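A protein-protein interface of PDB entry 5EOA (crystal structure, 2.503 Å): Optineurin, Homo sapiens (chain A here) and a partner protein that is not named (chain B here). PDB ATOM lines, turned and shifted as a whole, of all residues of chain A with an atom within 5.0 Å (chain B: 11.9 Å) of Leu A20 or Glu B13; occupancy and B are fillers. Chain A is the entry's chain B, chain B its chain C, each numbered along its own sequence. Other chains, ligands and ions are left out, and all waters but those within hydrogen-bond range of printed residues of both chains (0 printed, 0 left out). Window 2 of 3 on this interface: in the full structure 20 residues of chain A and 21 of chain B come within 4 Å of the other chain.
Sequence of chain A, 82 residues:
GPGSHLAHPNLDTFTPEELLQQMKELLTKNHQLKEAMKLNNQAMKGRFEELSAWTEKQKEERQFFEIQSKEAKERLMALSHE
Of the 17 printed residues of chain B, 6 touch a printed residue of chain A.
Among the printed residues, pairs that only touch across the chains: Leu A19 with Met B14, Leu A20 with Thr B10, Leu A20 with Glu B13, Leu A20 with Met B14, Met A23 with Met B14, Met A23 with Gly B17, Met A23 with Met B18 and Met A23 with Leu B21.
Printed residues of chain B within 4 Å of Leu A20: Thr B10, Glu B13 and Met B14. Of the printed residues of chain A, Glu B13 touches Leu A20 and Lys A24. Pro A16 touches none of the printed residues of chain B. No residue of chain B comes within 4 Å of Glu A17. Gln A21 touches none of the printed residues of chain B. Of chain B, only Met B14 (3.4 Å), Gly B17 (3.6 Å), Met B18 (3.7 Å) and Leu B21 (3.7 Å) come within 4 Å of Met A23. Of the printed residues of chain A, Leu B21 touches Met A23 (3.7 Å). Of the printed residues of chain B, Lys A24 touches Glu B13. Printed residues of chain A within 4 Å of Met B18: Met A23. Printed residues of chain A within 4 Å of Met B14: Leu A19 (3.6 Å), Leu A20 (3.6 Å) and Met A23 (3.4 Å). Printed residues of chain A within 4 Å of Gly B17: Met A23. Lys B22 touches none of the printed residues of chain A. The nearest printed residue of chain A that does not touch Leu B21 is Gln A22 (6.6 Å).
The side-chain hydroxyl (OG) of Ser B7 lies within hydrogen-bond range of the side-chain hydroxyl (OG1) of Thr B10 (3.0 Å).
The side-chain amino group of Lys A24 is in salt-bridge range of the side-chain carboxylate of Glu B13, at 3.8 Å.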
ATOM      1  N   PRO A  16     -19.130   5.147  22.032  1.00  0.00           N
ATOM      2  CA  PRO A  16     -19.564   6.247  22.909  1.00  0.00           C
ATOM      3  C   PRO A  16     -20.963   6.738  22.567  1.00  0.00           C
ATOM      4  O   PRO A  16     -21.728   7.065  23.468  1.00  0.00           O
ATOM      5  CB  PRO A  16     -18.548   7.348  22.617  1.00  0.00           C
ATOM      6  CG  PRO A  16     -17.336   6.610  22.139  1.00  0.00           C
ATOM      7  CD  PRO A  16     -17.845   5.442  21.370  1.00  0.00           C
ATOM      8  N   GLU A  17     -21.294   6.787  21.282  1.00  0.00           N
ATOM      9  CA  GLU A  17     -22.622   7.225  20.883  1.00  0.00           C
ATOM     10  C   GLU A  17     -23.674   6.230  21.367  1.00  0.00           C
ATOM     11  O   GLU A  17     -24.788   6.624  21.736  1.00  0.00           O
ATOM     12  CB  GLU A  17     -22.706   7.439  19.367  1.00  0.00           C
ATOM     13  CG  GLU A  17     -24.053   7.967  18.883  1.00  0.00           C
ATOM     14  CD  GLU A  17     -24.559   9.166  19.693  1.00  0.00           C
ATOM     15  OE1 GLU A  17     -25.460   8.983  20.547  1.00  0.00           O
ATOM     16  OE2 GLU A  17     -24.068  10.294  19.468  1.00  0.00           O
ATOM     17  N   GLU A  18     -23.310   4.947  21.387  1.00  0.00           N
ATOM     18  CA  GLU A  18     -24.214   3.898  21.862  1.00  0.00           C
ATOM     19  C   GLU A  18     -24.399   4.008  23.384  1.00  0.00           C
ATOM     20  O   GLU A  18     -25.486   3.788  23.916  1.00  0.00           O
ATOM     21  CB  GLU A  18     -23.691   2.515  21.461  1.00  0.00           C
ATOM     22  CG  GLU A  18     -23.697   2.261  19.947  1.00  0.00           C
ATOM     23  CD  GLU A  18     -23.095   0.912  19.555  1.00  0.00           C
ATOM     24  OE1 GLU A  18     -23.185   0.539  18.363  1.00  0.00           O
ATOM     25  OE2 GLU A  18     -22.525   0.230  20.431  1.00  0.00           O
ATOM     26  N   LEU A  19     -23.319   4.357  24.072  1.00  0.00           N
ATOM     27  CA  LEU A  19     -23.357   4.637  25.495  1.00  0.00           C
ATOM     28  C   LEU A  19     -24.341   5.758  25.798  1.00  0.00           C
ATOM     29  O   LEU A  19     -25.281   5.569  26.578  1.00  0.00           O
ATOM     30  CB  LEU A  19     -21.967   5.050  25.969  1.00  0.00           C
ATOM     31  CG  LEU A  19     -21.716   4.816  27.449  1.00  0.00           C
ATOM     32  CD1 LEU A  19     -21.646   3.335  27.721  1.00  0.00           C
ATOM     33  CD2 LEU A  19     -20.448   5.513  27.881  1.00  0.00           C
ATOM     34  N   LEU A  20     -24.113   6.926  25.193  1.00  0.00           N
ATOM     35  CA  LEU A  20     -25.028   8.059  25.341  1.00  0.00           C
ATOM     36  C   LEU A  20     -26.486   7.658  25.093  1.00  0.00           C
ATOM     37  O   LEU A  20     -27.378   8.045  25.844  1.00  0.00           O
ATOM     38  CB  LEU A  20     -24.635   9.200  24.411  1.00  0.00           C
ATOM     39  CG  LEU A  20     -23.385   9.968  24.819  1.00  0.00           C
ATOM     40  CD1 LEU A  20     -23.179  11.166  23.920  1.00  0.00           C
ATOM     41  CD2 LEU A  20     -23.503  10.412  26.261  1.00  0.00           C
ATOM     42  N   GLN A  21     -26.694   6.872  24.039  1.00  0.00           N
ATOM     43  CA  GLN A  21     -28.005   6.382  23.644  1.00  0.00           C
ATOM     44  C   GLN A  21     -28.687   5.606  24.778  1.00  0.00           C
ATOM     45  O   GLN A  21     -29.824   5.906  25.162  1.00  0.00           O
ATOM     46  CB  GLN A  21     -27.842   5.477  22.426  1.00  0.00           C
ATOM     47  CG  GLN A  21     -29.135   4.996  21.819  1.00  0.00           C
ATOM     48  CD  GLN A  21     -29.807   6.065  20.993  1.00  0.00           C
ATOM     49  OE1 GLN A  21     -29.264   6.515  19.978  1.00  0.00           O
ATOM     50  NE2 GLN A  21     -30.993   6.487  21.425  1.00  0.00           N
ATOM     51  N   GLN A  22     -27.975   4.607  25.294  1.00  0.00           N
ATOM     52  CA  GLN A  22     -28.420   3.823  26.436  1.00  0.00           C
ATOM     53  C   GLN A  22     -28.807   4.704  27.610  1.00  0.00           C
ATOM     54  O   GLN A  22     -29.817   4.475  28.247  1.00  0.00           O
ATOM     55  CB  GLN A  22     -27.325   2.850  26.859  1.00  0.00           C
ATOM     56  CG  GLN A  22     -27.253   1.639  25.975  1.00  0.00           C
ATOM     57  CD  GLN A  22     -28.539   0.847  26.001  1.00  0.00           C
ATOM     58  OE1 GLN A  22     -28.874   0.230  27.017  1.00  0.00           O
ATOM     59  NE2 GLN A  22     -29.285   0.877  24.890  1.00  0.00           N
ATOM     60  N   MET A  23     -27.999   5.720  27.869  1.00  0.00           N
ATOM     61  CA  MET A  23     -28.252   6.682  28.925  1.00  0.00           C
ATOM     62  C   MET A  23     -29.567   7.426  28.734  1.00  0.00           C
ATOM     63  O   MET A  23     -30.329   7.611  29.699  1.00  0.00           O
ATOM     64  CB  MET A  23     -27.095   7.679  29.006  1.00  0.00           C
ATOM     65  CG  MET A  23     -27.397   8.872  29.883  1.00  0.00           C
ATOM     66  SD  MET A  23     -27.578   8.408  31.617  1.00  0.00           S
ATOM     67  CE  MET A  23     -25.893   7.878  31.963  1.00  0.00           C
ATOM     68  N   LYS A  24     -29.830   7.854  27.501  1.00  0.00           N
ATOM     69  CA  LYS A  24     -31.058   8.581  27.201  1.00  0.00           C
ATOM     70  C   LYS A  24     -32.298   7.706  27.414  1.00  0.00           C
ATOM     71  O   LYS A  24     -33.291   8.146  27.997  1.00  0.00           O
ATOM     72  CB  LYS A  24     -31.020   9.143  25.780  1.00  0.00           C
ATOM     73  CG  LYS A  24     -29.986  10.240  25.602  1.00  0.00           C
ATOM     74  CD  LYS A  24     -30.425  11.235  24.539  1.00  0.00           C
ATOM     75  CE  LYS A  24     -29.461  12.409  24.467  1.00  0.00           C
ATOM     76  NZ  LYS A  24     -29.874  13.423  23.456  1.00  0.00           N
ATOM     77  N   PRO B   6     -13.717   8.028  25.677  1.00  0.00           N
ATOM     78  CA  PRO B   6     -14.149   9.098  26.577  1.00  0.00           C
ATOM     79  C   PRO B   6     -13.713  10.478  26.073  1.00  0.00           C
ATOM     80  O   PRO B   6     -12.521  10.802  26.141  1.00  0.00           O
ATOM     81  CB  PRO B   6     -13.415   8.765  27.884  1.00  0.00           C
ATOM     82  CG  PRO B   6     -12.359   7.704  27.518  1.00  0.00           C
ATOM     83  CD  PRO B   6     -12.374   7.546  26.029  1.00  0.00           C
ATOM     84  N   SER B   7     -14.660  11.271  25.570  1.00  0.00           N
ATOM     85  CA  SER B   7     -14.374  12.640  25.131  1.00  0.00           C
ATOM     86  C   SER B   7     -15.092  13.654  26.020  1.00  0.00           C
ATOM     87  O   SER B   7     -15.987  13.288  26.792  1.00  0.00           O
ATOM     88  CB  SER B   7     -14.768  12.852  23.662  1.00  0.00           C
ATOM     89  OG  SER B   7     -16.169  13.035  23.509  1.00  0.00           O
ATOM     90  N   SER B   8     -14.692  14.920  25.911  1.00  0.00           N
ATOM     91  CA  SER B   8     -15.294  15.989  26.703  1.00  0.00           C
ATOM     92  C   SER B   8     -16.816  16.005  26.544  1.00  0.00           C
ATOM     93  O   SER B   8     -17.546  15.783  27.513  1.00  0.00           O
ATOM     94  CB  SER B   8     -14.698  17.347  26.327  1.00  0.00           C
ATOM     95  OG  SER B   8     -15.143  18.357  27.215  1.00  0.00           O
ATOM     96  N   ASN B   9     -17.279  16.243  25.317  1.00  0.00           N
ATOM     97  CA  ASN B   9     -18.707  16.276  25.011  1.00  0.00           C
ATOM     98  C   ASN B   9     -19.449  15.062  25.571  1.00  0.00           C
ATOM     99  O   ASN B   9     -20.487  15.205  26.224  1.00  0.00           O
ATOM    100  CB  ASN B   9     -18.924  16.390  23.500  1.00  0.00           C
ATOM    101  CG  ASN B   9     -20.388  16.567  23.130  1.00  0.00           C
ATOM    102  OD1 ASN B   9     -21.148  15.594  23.061  1.00  0.00           O
ATOM    103  ND2 ASN B   9     -20.790  17.808  22.876  1.00  0.00           N
ATOM    104  N   THR B  10     -18.891  13.876  25.336  1.00  0.00           N
ATOM    105  CA  THR B  10     -19.500  12.625  25.782  1.00  0.00           C
ATOM    106  C   THR B  10     -19.581  12.526  27.310  1.00  0.00           C
ATOM    107  O   THR B  10     -20.620  12.168  27.853  1.00  0.00           O
ATOM    108  CB  THR B  10     -18.760  11.405  25.190  1.00  0.00           C
ATOM    109  OG1 THR B  10     -18.738  11.526  23.765  1.00  0.00           O
ATOM    110  CG2 THR B  10     -19.463  10.108  25.557  1.00  0.00           C
ATOM    111  N   LEU B  11     -18.486  12.866  27.987  1.00  0.00           N
ATOM    112  CA  LEU B  11     -18.427  12.834  29.442  1.00  0.00           C
ATOM    113  C   LEU B  11     -19.371  13.838  30.068  1.00  0.00           C
ATOM    114  O   LEU B  11     -19.967  13.568  31.106  1.00  0.00           O
ATOM    115  CB  LEU B  11     -17.006  13.119  29.928  1.00  0.00           C
ATOM    116  CG  LEU B  11     -16.008  11.989  29.711  1.00  0.00           C
ATOM    117  CD1 LEU B  11     -14.713  12.250  30.445  1.00  0.00           C
ATOM    118  CD2 LEU B  11     -16.617  10.698  30.166  1.00  0.00           C
ATOM    119  N   VAL B  12     -19.493  15.000  29.442  1.00  0.00           N
ATOM    120  CA  VAL B  12     -20.367  16.041  29.946  1.00  0.00           C
ATOM    121  C   VAL B  12     -21.787  15.535  29.901  1.00  0.00           C
ATOM    122  O   VAL B  12     -22.500  15.562  30.912  1.00  0.00           O
ATOM    123  CB  VAL B  12     -20.224  17.327  29.121  1.00  0.00           C
ATOM    124  CG1 VAL B  12     -21.458  18.210  29.275  1.00  0.00           C
ATOM    125  CG2 VAL B  12     -18.974  18.054  29.533  1.00  0.00           C
ATOM    126  N   GLU B  13     -22.179  15.037  28.731  1.00  0.00           N
ATOM    127  CA  GLU B  13     -23.518  14.488  28.554  1.00  0.00           C
ATOM    128  C   GLU B  13     -23.702  13.242  29.419  1.00  0.00           C
ATOM    129  O   GLU B  13     -24.781  13.003  29.940  1.00  0.00           O
ATOM    130  CB  GLU B  13     -23.791  14.181  27.080  1.00  0.00           C
ATOM    131  CG  GLU B  13     -25.252  13.919  26.779  1.00  0.00           C
ATOM    132  CD  GLU B  13     -25.499  13.616  25.321  1.00  0.00           C
ATOM    133  OE1 GLU B  13     -26.465  12.876  25.026  1.00  0.00           O
ATOM    134  OE2 GLU B  13     -24.731  14.124  24.472  1.00  0.00           O
ATOM    135  N   MET B  14     -22.636  12.468  29.580  1.00  0.00           N
ATOM    136  CA  MET B  14     -22.649  11.296  30.440  1.00  0.00           C
ATOM    137  C   MET B  14     -22.819  11.704  31.902  1.00  0.00           C
ATOM    138  O   MET B  14     -23.567  11.070  32.656  1.00  0.00           O
ATOM    139  CB  MET B  14     -21.348  10.510  30.264  1.00  0.00           C
ATOM    140  CG  MET B  14     -21.534   9.024  30.299  1.00  0.00           C
ATOM    141  SD  MET B  14     -22.871   8.503  29.207  1.00  0.00           S
ATOM    142  CE  MET B  14     -23.277   6.927  29.964  1.00  0.00           C
ATOM    143  N   THR B  15     -22.130  12.772  32.297  1.00  0.00           N
ATOM    144  CA  THR B  15     -22.211  13.256  33.670  1.00  0.00           C
ATOM    145  C   THR B  15     -23.602  13.826  33.938  1.00  0.00           C
ATOM    146  O   THR B  15     -24.159  13.628  35.006  1.00  0.00           O
ATOM    147  CB  THR B  15     -21.148  14.336  33.954  1.00  0.00           C
ATOM    148  OG1 THR B  15     -19.838  13.788  33.764  1.00  0.00           O
ATOM    149  CG2 THR B  15     -21.265  14.837  35.380  1.00  0.00           C
ATOM    150  N   LEU B  16     -24.162  14.523  32.955  1.00  0.00           N
ATOM    151  CA  LEU B  16     -25.479  15.143  33.092  1.00  0.00           C
ATOM    152  C   LEU B  16     -26.561  14.068  33.235  1.00  0.00           C
ATOM    153  O   LEU B  16     -27.471  14.178  34.073  1.00  0.00           O
ATOM    154  CB  LEU B  16     -25.765  16.020  31.870  1.00  0.00           C
ATOM    155  CG  LEU B  16     -26.805  17.142  31.940  1.00  0.00           C
ATOM    156  CD1 LEU B  16     -26.247  18.362  32.657  1.00  0.00           C
ATOM    157  CD2 LEU B  16     -27.274  17.518  30.543  1.00  0.00           C
ATOM    158  N   GLY B  17     -26.459  13.025  32.416  1.00  0.00           N
ATOM    159  CA  GLY B  17     -27.380  11.919  32.506  1.00  0.00           C
ATOM    160  C   GLY B  17     -27.284  11.240  33.859  1.00  0.00           C
ATOM    161  O   GLY B  17     -28.308  10.929  34.489  1.00  0.00           O
ATOM    162  N   MET B  18     -26.055  11.022  34.313  1.00  0.00           N
ATOM    163  CA  MET B  18     -25.819  10.276  35.539  1.00  0.00           C
ATOM    164  C   MET B  18     -26.418  10.994  36.731  1.00  0.00           C
ATOM    165  O   MET B  18     -27.106  10.378  37.560  1.00  0.00           O
ATOM    166  CB  MET B  18     -24.321  10.074  35.745  1.00  0.00           C
ATOM    167  CG  MET B  18     -24.000   8.749  36.376  1.00  0.00           C
ATOM    168  SD  MET B  18     -24.659   7.362  35.418  1.00  0.00           S
ATOM    169  CE  MET B  18     -24.464   6.075  36.608  1.00  0.00           C
ATOM    170  N   LYS B  19     -26.175  12.301  36.802  1.00  0.00           N
ATOM    171  CA  LYS B  19     -26.729  13.113  37.879  1.00  0.00           C
ATOM    172  C   LYS B  19     -28.262  13.104  37.865  1.00  0.00           C
ATOM    173  O   LYS B  19     -28.898  13.086  38.909  1.00  0.00           O
ATOM    174  CB  LYS B  19     -26.175  14.536  37.815  1.00  0.00           C
ATOM    175  CG  LYS B  19     -24.681  14.608  38.110  1.00  0.00           C
ATOM    176  CD  LYS B  19     -24.149  16.053  38.128  1.00  0.00           C
ATOM    177  CE  LYS B  19     -22.680  16.093  38.531  1.00  0.00           C
ATOM    178  NZ  LYS B  19     -22.107  17.475  38.566  1.00  0.00           N
ATOM    179  N   LYS B  20     -28.842  13.096  36.672  1.00  0.00           N
ATOM    180  CA  LYS B  20     -30.284  13.101  36.528  1.00  0.00           C
ATOM    181  C   LYS B  20     -30.857  11.784  37.009  1.00  0.00           C
ATOM    182  O   LYS B  20     -31.855  11.764  37.721  1.00  0.00           O
ATOM    183  CB  LYS B  20     -30.653  13.304  35.069  1.00  0.00           C
ATOM    184  CG  LYS B  20     -31.851  14.208  34.849  1.00  0.00           C
ATOM    185  CD  LYS B  20     -33.101  13.728  35.571  1.00  0.00           C
ATOM    186  CE  LYS B  20     -34.193  14.770  35.473  1.00  0.00           C
ATOM    187  NZ  LYS B  20     -34.394  15.199  34.063  1.00  0.00           N
ATOM    188  N   LEU B  21     -30.229  10.687  36.607  1.00  0.00           N
ATOM    189  CA  LEU B  21     -30.678   9.364  37.019  1.00  0.00           C
ATOM    190  C   LEU B  21     -30.604   9.237  38.534  1.00  0.00           C
ATOM    191  O   LEU B  21     -31.499   8.676  39.159  1.00  0.00           O
ATOM    192  CB  LEU B  21     -29.813   8.294  36.358  1.00  0.00           C
ATOM    193  CG  LEU B  21     -30.477   7.336  35.364  1.00  0.00           C
ATOM    194  CD1 LEU B  21     -31.623   7.984  34.635  1.00  0.00           C
ATOM    195  CD2 LEU B  21     -29.451   6.838  34.371  1.00  0.00           C
ATOM    196  N   LYS B  22     -29.534   9.780  39.110  1.00  0.00           N
ATOM    197  CA  LYS B  22     -29.305   9.726  40.544  1.00  0.00           C
ATOM    198  C   LYS B  22     -30.410  10.486  41.277  1.00  0.00           C
ATOM    199  O   LYS B  22     -30.978  10.013  42.273  1.00  0.00           O
ATOM    200  CB  LYS B  22     -27.941  10.344  40.848  1.00  0.00           C
ATOM    201  CG  LYS B  22     -27.078   9.529  41.784  1.00  0.00           C
ATOM    202  CD  LYS B  22     -27.326   9.907  43.233  1.00  0.00           C
ATOM    203  CE  LYS B  22     -26.526  11.134  43.622  1.00  0.00           C
ATOM    204  NZ  LYS B  22     -25.072  10.825  43.657  1.00  0.00           N
